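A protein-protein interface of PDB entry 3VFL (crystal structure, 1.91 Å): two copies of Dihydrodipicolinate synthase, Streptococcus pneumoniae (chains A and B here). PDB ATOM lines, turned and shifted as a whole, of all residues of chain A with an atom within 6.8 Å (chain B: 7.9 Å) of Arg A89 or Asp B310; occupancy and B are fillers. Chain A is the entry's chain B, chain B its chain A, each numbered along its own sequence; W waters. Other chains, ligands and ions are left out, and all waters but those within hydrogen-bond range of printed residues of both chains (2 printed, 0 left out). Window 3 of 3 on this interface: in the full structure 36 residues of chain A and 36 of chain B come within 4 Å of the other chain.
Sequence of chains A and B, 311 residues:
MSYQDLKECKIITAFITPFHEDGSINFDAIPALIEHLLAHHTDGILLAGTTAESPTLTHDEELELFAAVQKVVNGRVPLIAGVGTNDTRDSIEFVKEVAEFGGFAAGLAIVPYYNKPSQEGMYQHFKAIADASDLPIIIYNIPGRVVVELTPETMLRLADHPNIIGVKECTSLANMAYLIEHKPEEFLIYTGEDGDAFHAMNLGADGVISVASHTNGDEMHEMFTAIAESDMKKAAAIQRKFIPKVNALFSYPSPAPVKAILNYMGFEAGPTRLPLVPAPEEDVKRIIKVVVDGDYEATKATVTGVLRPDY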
ATOM      1  N   THR A  85      15.106   6.840   1.628  1.00  0.00           N
ATOM      2  CA  THR A  85      15.565   7.854   0.727  1.00  0.00           C
ATOM      3  C   THR A  85      14.389   8.757   0.362  1.00  0.00           C
ATOM      4  O   THR A  85      13.319   8.732   1.030  1.00  0.00           O
ATOM      5  CB  THR A  85      16.137   7.260  -0.614  1.00  0.00           C
ATOM      6  OG1 THR A  85      15.044   6.755  -1.408  1.00  0.00           O
ATOM      7  CG2 THR A  85      17.152   6.156  -0.361  1.00  0.00           C
ATOM      8  N   ASN A  86      14.550   9.580  -0.661  1.00  0.00           N
ATOM      9  CA  ASN A  86      13.508  10.488  -1.018  1.00  0.00           C
ATOM     10  C   ASN A  86      12.541   9.886  -2.049  1.00  0.00           C
ATOM     11  O   ASN A  86      11.704  10.605  -2.636  1.00  0.00           O
ATOM     12  CB  ASN A  86      14.039  11.882  -1.478  1.00  0.00           C
ATOM     13  CG  ASN A  86      14.780  11.852  -2.799  1.00  0.00           C
ATOM     14  OD1 ASN A  86      15.252  10.810  -3.288  1.00  0.00           O
ATOM     15  ND2 ASN A  86      14.897  12.999  -3.379  1.00  0.00           N
ATOM     16  N   ASP A  87      12.699   8.603  -2.297  1.00  0.00           N
ATOM     17  CA  ASP A  87      11.713   7.910  -3.122  1.00  0.00           C
ATOM     18  C   ASP A  87      10.958   6.904  -2.266  1.00  0.00           C
ATOM     19  O   ASP A  87      11.562   6.063  -1.624  1.00  0.00           O
ATOM     20  CB  ASP A  87      12.350   7.225  -4.313  1.00  0.00           C
ATOM     21  CG  ASP A  87      11.325   6.458  -5.121  1.00  0.00           C
ATOM     22  OD1 ASP A  87      10.312   7.065  -5.452  1.00  0.00           O
ATOM     23  OD2 ASP A  87      11.515   5.253  -5.362  1.00  0.00           O
ATOM     24  N   THR A  88       9.629   7.007  -2.237  1.00  0.00           N
ATOM     25  CA  THR A  88       8.878   6.162  -1.299  1.00  0.00           C
ATOM     26  C   THR A  88       8.915   4.694  -1.684  1.00  0.00           C
ATOM     27  O   THR A  88       9.136   3.791  -0.804  1.00  0.00           O
ATOM     28  CB  THR A  88       7.440   6.630  -1.109  1.00  0.00           C
ATOM     29  OG1 THR A  88       7.456   8.005  -0.753  1.00  0.00           O
ATOM     30  CG2 THR A  88       6.739   5.850   0.087  1.00  0.00           C
ATOM     31  N   ARG A  89       8.774   4.413  -2.982  1.00  0.00           N
ATOM     32  CA  ARG A  89       8.896   2.991  -3.409  1.00  0.00           C
ATOM     33  C   ARG A  89      10.245   2.318  -3.029  1.00  0.00           C
ATOM     34  O   ARG A  89      10.230   1.189  -2.510  1.00  0.00           O
ATOM     35  CB  ARG A  89       8.635   2.814  -4.944  1.00  0.00           C
ATOM     36  CG  ARG A  89       9.017   1.430  -5.485  1.00  0.00           C
ATOM     37  CD  ARG A  89       8.144   0.255  -5.015  1.00  0.00           C
ATOM     38  NE  ARG A  89       6.721   0.481  -5.240  1.00  0.00           N
ATOM     39  CZ  ARG A  89       5.734  -0.094  -4.545  1.00  0.00           C
ATOM     40  NH1 ARG A  89       5.969  -0.922  -3.565  1.00  0.00           N
ATOM     41  NH2 ARG A  89       4.482   0.203  -4.814  1.00  0.00           N
ATOM     42  N   ASP A  90      11.383   2.974  -3.319  1.00  0.00           N
ATOM     43  CA  ASP A  90      12.745   2.467  -2.987  1.00  0.00           C
ATOM     44  C   ASP A  90      12.884   2.222  -1.514  1.00  0.00           C
ATOM     45  O   ASP A  90      13.389   1.170  -1.057  1.00  0.00           O
ATOM     46  CB  ASP A  90      13.894   3.403  -3.406  1.00  0.00           C
ATOM     47  CG  ASP A  90      14.082   3.493  -4.925  1.00  0.00           C
ATOM     48  OD1 ASP A  90      13.524   2.628  -5.647  1.00  0.00           O
ATOM     49  OD2 ASP A  90      14.798   4.436  -5.411  1.00  0.00           O
ATOM     50  N   SER A  91      12.388   3.166  -0.739  1.00  0.00           N
ATOM     51  CA  SER A  91      12.450   2.999   0.688  1.00  0.00           C
ATOM     52  C   SER A  91      11.698   1.748   1.166  1.00  0.00           C
ATOM     53  O   SER A  91      12.146   1.085   2.111  1.00  0.00           O
ATOM     54  CB  SER A  91      11.879   4.247   1.381  1.00  0.00           C
ATOM     55  OG  SER A  91      12.607   5.420   1.030  1.00  0.00           O
ATOM     56  N   ILE A  92      10.498   1.526   0.620  1.00  0.00           N
ATOM     57  CA  ILE A  92       9.674   0.304   0.906  1.00  0.00           C
ATOM     58  C   ILE A  92      10.450  -0.949   0.545  1.00  0.00           C
ATOM     59  O   ILE A  92      10.591  -1.886   1.370  1.00  0.00           O
ATOM     60  CB  ILE A  92       8.323   0.303   0.123  1.00  0.00           C
ATOM     61  CG1 ILE A  92       7.360   1.329   0.710  1.00  0.00           C
ATOM     62  CG2 ILE A  92       7.568  -1.011   0.390  1.00  0.00           C
ATOM     63  CD1 ILE A  92       6.318   1.835  -0.266  1.00  0.00           C
ATOM     64  N   GLU A  93      11.009  -0.961  -0.661  1.00  0.00           N
ATOM     65  CA  GLU A  93      11.712  -2.158  -1.145  1.00  0.00           C
ATOM     66  C   GLU A  93      12.962  -2.355  -0.292  1.00  0.00           C
ATOM     67  O   GLU A  93      13.343  -3.457  -0.027  1.00  0.00           O
ATOM     68  CB  GLU A  93      12.067  -2.096  -2.661  1.00  0.00           C
ATOM     69  CG  GLU A  93      10.853  -2.133  -3.652  1.00  0.00           C
ATOM     70  CD  GLU A  93       9.623  -2.993  -3.219  1.00  0.00           C
ATOM     71  OE1 GLU A  93       9.690  -4.229  -3.184  1.00  0.00           O
ATOM     72  OE2 GLU A  93       8.527  -2.440  -2.934  1.00  0.00           O
ATOM     73  N   PHE A  94      13.626  -1.294   0.153  1.00  0.00           N
ATOM     74  CA  PHE A  94      14.834  -1.520   0.939  1.00  0.00           C
ATOM     75  C   PHE A  94      14.497  -1.937   2.397  1.00  0.00           C
ATOM     76  O   PHE A  94      15.205  -2.770   2.974  1.00  0.00           O
ATOM     77  CB  PHE A  94      15.819  -0.312   0.817  1.00  0.00           C
ATOM     78  CG  PHE A  94      17.185  -0.583   1.364  1.00  0.00           C
ATOM     79  CD1 PHE A  94      18.015  -1.583   0.796  1.00  0.00           C
ATOM     80  CD2 PHE A  94      17.684   0.165   2.435  1.00  0.00           C
ATOM     81  CE1 PHE A  94      19.277  -1.818   1.295  1.00  0.00           C
ATOM     82  CE2 PHE A  94      18.968  -0.084   2.929  1.00  0.00           C
ATOM     83  CZ  PHE A  94      19.763  -1.066   2.367  1.00  0.00           C
ATOM     84  N   LYS A  96      12.204  -3.768   3.356  1.00  0.00           N
ATOM     85  CA  LYS A  96      11.832  -5.183   3.278  1.00  0.00           C
ATOM     86  C   LYS A  96      13.078  -5.992   3.205  1.00  0.00           C
ATOM     87  O   LYS A  96      13.269  -6.897   4.020  1.00  0.00           O
ATOM     88  CB  LYS A  96      10.963  -5.427   2.080  1.00  0.00           C
ATOM     89  CG  LYS A  96       9.553  -4.950   2.306  1.00  0.00           C
ATOM     90  CD  LYS A  96       8.706  -5.402   1.138  1.00  0.00           C
ATOM     91  CE  LYS A  96       7.254  -5.410   1.545  1.00  0.00           C
ATOM     92  NZ  LYS A  96       6.496  -4.844   0.398  1.00  0.00           N
ATOM     93  N   HIS A 125       4.363   8.835   2.899  1.00  0.00           N
ATOM     94  CA  HIS A 125       5.671   8.300   2.817  1.00  0.00           C
ATOM     95  C   HIS A 125       6.057   7.416   3.992  1.00  0.00           C
ATOM     96  O   HIS A 125       6.346   6.184   3.819  1.00  0.00           O
ATOM     97  CB  HIS A 125       6.624   9.486   2.704  1.00  0.00           C
ATOM     98  CG  HIS A 125       8.049   9.079   2.654  1.00  0.00           C
ATOM     99  ND1 HIS A 125       8.583   8.494   1.596  1.00  0.00           N
ATOM    100  CD2 HIS A 125       9.069   9.163   3.616  1.00  0.00           C
ATOM    101  CE1 HIS A 125       9.858   8.232   1.831  1.00  0.00           C
ATOM    102  NE2 HIS A 125      10.143   8.657   3.074  1.00  0.00           N
ATOM    103  N   ASP B  22      -2.493   4.728 -11.376  1.00  0.00           N
ATOM    104  CA  ASP B  22      -1.865   3.453 -11.140  1.00  0.00           C
ATOM    105  C   ASP B  22      -0.359   3.538 -10.736  1.00  0.00           C
ATOM    106  O   ASP B  22       0.198   2.634 -10.112  1.00  0.00           O
ATOM    107  CB  ASP B  22      -2.220   2.733 -12.439  1.00  0.00           C
ATOM    108  CG  ASP B  22      -1.117   1.994 -13.075  1.00  0.00           C
ATOM    109  OD1 ASP B  22      -1.396   0.808 -13.243  1.00  0.00           O
ATOM    110  OD2 ASP B  22      -0.092   2.564 -13.521  1.00  0.00           O
ATOM    111  N   PRO B  55      13.389  12.211  -8.658  1.00  0.00           N
ATOM    112  CA  PRO B  55      13.756  11.347  -7.538  1.00  0.00           C
ATOM    113  C   PRO B  55      13.019  10.004  -7.502  1.00  0.00           C
ATOM    114  O   PRO B  55      13.546   9.037  -6.983  1.00  0.00           O
ATOM    115  CB  PRO B  55      13.350  12.202  -6.329  1.00  0.00           C
ATOM    116  CG  PRO B  55      13.537  13.575  -6.807  1.00  0.00           C
ATOM    117  CD  PRO B  55      12.956  13.547  -8.187  1.00  0.00           C
ATOM    118  N   THR B  56      11.842   9.945  -8.091  1.00  0.00           N
ATOM    119  CA  THR B  56      10.964   8.760  -8.091  1.00  0.00           C
ATOM    120  C   THR B  56      11.008   8.016  -9.481  1.00  0.00           C
ATOM    121  O   THR B  56      10.349   6.954  -9.668  1.00  0.00           O
ATOM    122  CB  THR B  56       9.512   9.159  -7.812  1.00  0.00           C
ATOM    123  OG1 THR B  56       8.960   9.857  -8.967  1.00  0.00           O
ATOM    124  CG2 THR B  56       9.359  10.113  -6.518  1.00  0.00           C
ATOM    125  N   THR B  58      12.695   5.592 -12.082  1.00  0.00           N
ATOM    126  CA  THR B  58      13.858   4.708 -12.205  1.00  0.00           C
ATOM    127  C   THR B  58      14.828   5.017 -13.338  1.00  0.00           C
ATOM    128  O   THR B  58      14.517   5.791 -14.248  1.00  0.00           O
ATOM    129  CB  THR B  58      13.483   3.210 -12.292  1.00  0.00           C
ATOM    130  OG1 THR B  58      12.750   2.971 -13.493  1.00  0.00           O
ATOM    131  CG2 THR B  58      12.643   2.790 -11.097  1.00  0.00           C
ATOM    132  N   ARG B 273       3.868  10.811  -7.664  1.00  0.00           N
ATOM    133  CA  ARG B 273       4.411   9.690  -6.967  1.00  0.00           C
ATOM    134  C   ARG B 273       4.900  10.109  -5.546  1.00  0.00           C
ATOM    135  O   ARG B 273       5.595  11.149  -5.342  1.00  0.00           O
ATOM    136  CB  ARG B 273       5.558   9.131  -7.751  1.00  0.00           C
ATOM    137  CG  ARG B 273       5.140   8.228  -8.895  1.00  0.00           C
ATOM    138  CD  ARG B 273       6.402   7.699  -9.506  1.00  0.00           C
ATOM    139  NE  ARG B 273       6.001   6.694 -10.507  1.00  0.00           N
ATOM    140  CZ  ARG B 273       6.815   6.070 -11.317  1.00  0.00           C
ATOM    141  NH1 ARG B 273       8.111   6.323 -11.299  1.00  0.00           N
ATOM    142  NH2 ARG B 273       6.311   5.134 -12.151  1.00  0.00           N
ATOM    143  N   LEU B 274       4.506   9.338  -4.549  1.00  0.00           N
ATOM    144  CA  LEU B 274       5.029   9.606  -3.206  1.00  0.00           C
ATOM    145  C   LEU B 274       6.562   9.721  -3.186  1.00  0.00           C
ATOM    146  O   LEU B 274       7.290   8.969  -3.884  1.00  0.00           O
ATOM    147  CB  LEU B 274       4.541   8.552  -2.260  1.00  0.00           C
ATOM    148  CG  LEU B 274       3.071   8.488  -1.966  1.00  0.00           C
ATOM    149  CD1 LEU B 274       2.986   7.168  -1.228  1.00  0.00           C
ATOM    150  CD2 LEU B 274       2.477   9.626  -1.118  1.00  0.00           C
ATOM    151  N   PRO B 275       7.110  10.617  -2.324  1.00  0.00           N
ATOM    152  CA  PRO B 275       6.474  11.322  -1.229  1.00  0.00           C
ATOM    153  C   PRO B 275       5.682  12.566  -1.598  1.00  0.00           C
ATOM    154  O   PRO B 275       5.210  13.264  -0.696  1.00  0.00           O
ATOM    155  CB  PRO B 275       7.672  11.669  -0.285  1.00  0.00           C
ATOM    156  CG  PRO B 275       8.826  11.829  -1.261  1.00  0.00           C
ATOM    157  CD  PRO B 275       8.583  10.741  -2.292  1.00  0.00           C
ATOM    158  N   VAL B 306       0.826   8.173  -5.190  1.00  0.00           N
ATOM    159  CA  VAL B 306       0.792   6.850  -5.794  1.00  0.00           C
ATOM    160  C   VAL B 306       2.210   6.313  -5.762  1.00  0.00           C
ATOM    161  O   VAL B 306       3.175   7.075  -5.651  1.00  0.00           O
ATOM    162  CB  VAL B 306       0.159   6.958  -7.240  1.00  0.00           C
ATOM    163  CG1 VAL B 306       0.267   5.685  -8.030  1.00  0.00           C
ATOM    164  CG2 VAL B 306      -1.325   7.304  -7.143  1.00  0.00           C
ATOM    165  N   LEU B 307       2.346   4.991  -5.822  1.00  0.00           N
ATOM    166  CA  LEU B 307       3.616   4.314  -5.907  1.00  0.00           C
ATOM    167  C   LEU B 307       3.762   3.640  -7.245  1.00  0.00           C
ATOM    168  O   LEU B 307       2.779   3.186  -7.868  1.00  0.00           O
ATOM    169  CB  LEU B 307       3.790   3.304  -4.781  1.00  0.00           C
ATOM    170  CG  LEU B 307       3.663   3.792  -3.352  1.00  0.00           C
ATOM    171  CD1 LEU B 307       3.365   2.592  -2.464  1.00  0.00           C
ATOM    172  CD2 LEU B 307       4.997   4.442  -2.966  1.00  0.00           C
ATOM    173  N   ARG B 308       4.983   3.641  -7.739  1.00  0.00           N
ATOM    174  CA  ARG B 308       5.227   2.945  -8.978  1.00  0.00           C
ATOM    175  C   ARG B 308       5.112   1.442  -8.767  1.00  0.00           C
ATOM    176  O   ARG B 308       5.617   0.912  -7.758  1.00  0.00           O
ATOM    177  CB  ARG B 308       6.537   3.315  -9.572  1.00  0.00           C
ATOM    178  CG  ARG B 308       7.775   2.760  -8.921  1.00  0.00           C
ATOM    179  CD  ARG B 308       8.796   2.591 -10.022  1.00  0.00           C
ATOM    180  NE  ARG B 308      10.171   2.425  -9.532  1.00  0.00           N
ATOM    181  CZ  ARG B 308      10.559   1.528  -8.625  1.00  0.00           C
ATOM    182  NH1 ARG B 308       9.668   0.706  -8.087  1.00  0.00           N
ATOM    183  NH2 ARG B 308      11.824   1.456  -8.225  1.00  0.00           N
ATOM    184  N   PRO B 309       4.433   0.750  -9.708  1.00  0.00           N
ATOM    185  CA  PRO B 309       4.114  -0.659  -9.534  1.00  0.00           C
ATOM    186  C   PRO B 309       5.214  -1.545  -8.986  1.00  0.00           C
ATOM    187  O   PRO B 309       6.353  -1.524  -9.446  1.00  0.00           O
ATOM    188  CB  PRO B 309       3.730  -1.069 -10.967  1.00  0.00           C
ATOM    189  CG  PRO B 309       2.932   0.112 -11.377  1.00  0.00           C
ATOM    190  CD  PRO B 309       3.950   1.203 -11.029  1.00  0.00           C
ATOM    191  N   ASP B 310       4.817  -2.296  -7.972  1.00  0.00           N
ATOM    192  CA  ASP B 310       5.553  -3.351  -7.290  1.00  0.00           C
ATOM    193  C   ASP B 310       5.918  -4.559  -8.208  1.00  0.00           C
ATOM    194  O   ASP B 310       6.521  -5.527  -7.766  1.00  0.00           O
ATOM    195  CB  ASP B 310       4.569  -3.829  -6.198  1.00  0.00           C
ATOM    196  CG  ASP B 310       5.232  -4.535  -5.067  1.00  0.00           C
ATOM    197  OD1 ASP B 310       6.474  -4.435  -4.947  1.00  0.00           O
ATOM    198  OD2 ASP B 310       4.497  -5.202  -4.282  1.00  0.00           O
ATOM    199  N   TYR B 311       5.564  -4.492  -9.490  1.00  0.00           N
ATOM    200  CA  TYR B 311       5.520  -5.676 -10.341  1.00  0.00           C
ATOM    201  C   TYR B 311       5.675  -5.236 -11.797  1.00  0.00           C
ATOM    202  O   TYR B 311       5.481  -4.065 -12.156  1.00  0.00           O
ATOM    203  CB  TYR B 311       4.164  -6.366 -10.126  1.00  0.00           C
ATOM    204  CG  TYR B 311       3.031  -5.371 -10.347  1.00  0.00           C
ATOM    205  CD1 TYR B 311       2.591  -5.052 -11.661  1.00  0.00           C
ATOM    206  CD2 TYR B 311       2.465  -4.666  -9.274  1.00  0.00           C
ATOM    207  CE1 TYR B 311       1.603  -4.111 -11.881  1.00  0.00           C
ATOM    208  CE2 TYR B 311       1.453  -3.729  -9.490  1.00  0.00           C
ATOM    209  CZ  TYR B 311       1.026  -3.464 -10.786  1.00  0.00           C
ATOM    210  OH  TYR B 311       0.043  -2.537 -11.018  1.00  0.00           O
ATOM    211  OXT TYR B 311       5.990  -6.051 -12.669  1.00  0.00           O
HETATM  212  O   HOH W   1      15.315   8.795  -4.977  1.00  0.00           O
HETATM  213  O   HOH W   2       6.257  -3.599  -2.085  1.00  0.00           O
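The side-chain hydroxyl of Thr A88 sits close to the backbone carbonyl oxygen of Leu B274 (3.3 Å).
OG1 of Thr A88 lies close to N of Pro B275, at 3.1 Å.
NE of Arg A89 sits at hydrogen-bond distance from O of Arg B308, at 2.8 Å.
The guanidinium group (NH2) of Arg B308 lies within salt-bridge range of the side-chain carboxylate (OD1) of Asp A90, 3.3 Å away.
OE2 of Glu A93 sits close to OD1 of Asp B310, at 3.5 Å.
NH1 of Arg A89 is in salt-bridge range of OD1 of Asp B310 (3.8 Å).
The backbone carbonyl oxygen of Asp A87 lies within hydrogen-bond range of the side-chain hydroxyl of Ser A91.
NH1 of Arg A89 is in salt-bridge range of OE2 of Glu A93 (3.0 Å).
N of Leu B274 sits at hydrogen-bond distance from O of Val B306.
The side-chain hydroxyl (OG1) of Thr A88 is in hydrogen-bond range of a ring nitrogen (ND1) of His A125 (2.7 Å).
The backbone carbonyl oxygen of Thr B56 is in hydrogen-bond range of the guanidinium group of Arg B273, 2.8 Å away.
N of Asp A90 sits at hydrogen-bond distance from OD2 of Asp A87 (3.1 Å).
Among the printed residues, pairs that only touch across the chains: Asn A86 with Pro B275, Arg A89 with Leu B307, Asp A87 with Thr B56, Asn A86 with Pro B55, Asp A87 with Pro B55, Ile A92 with Leu B307, Thr A88 with Leu B307, His A125 with Pro B275 and Asp A87 with Leu B274.
Arg A89 touches just these residues of chain B: Leu B307 (3.2 Å), Arg B308 (2.8 Å) and Asp B310 (3.8 Å).
Of the printed residues of chain B, His A125 touches Pro B275.
Printed residues of chain A within 4 Å of Pro B275: Asn A86, Thr A88 and His A125.
Hydrophobic or aromatic side chains of chain A within 4 Å of the printed part of chain B: Ile A92 and His A125.
Of the 13 printed residues of chain B, 7 touch a printed residue of chain A.
Hydrophobic or aromatic side chains of chain B that line the printed part of chain A: Pro B55, Leu B274, Pro B275 and Leu B307.
Along chain B the printed residues that touch a printed residue of chain A span positions 55 to 310.
Among the printed residues, 15 pairs touch across the chains.
No position is printed for both chains.
Of the 15 pairs that touch across the chains among the printed residues, none has its exchanged pair printed and touching as well.
Water W1 bridges OD1 of Asn A86 and O of Pro B55.
Water W2 lies within hydrogen-bond range of the side-chain carboxylate (OE2) of Glu A93, the side-chain amino group (NZ) of Lys A96, the side-chain carboxylate (OD1) of Asp B310 and the guanidinium group (NH1) of Arg A89.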
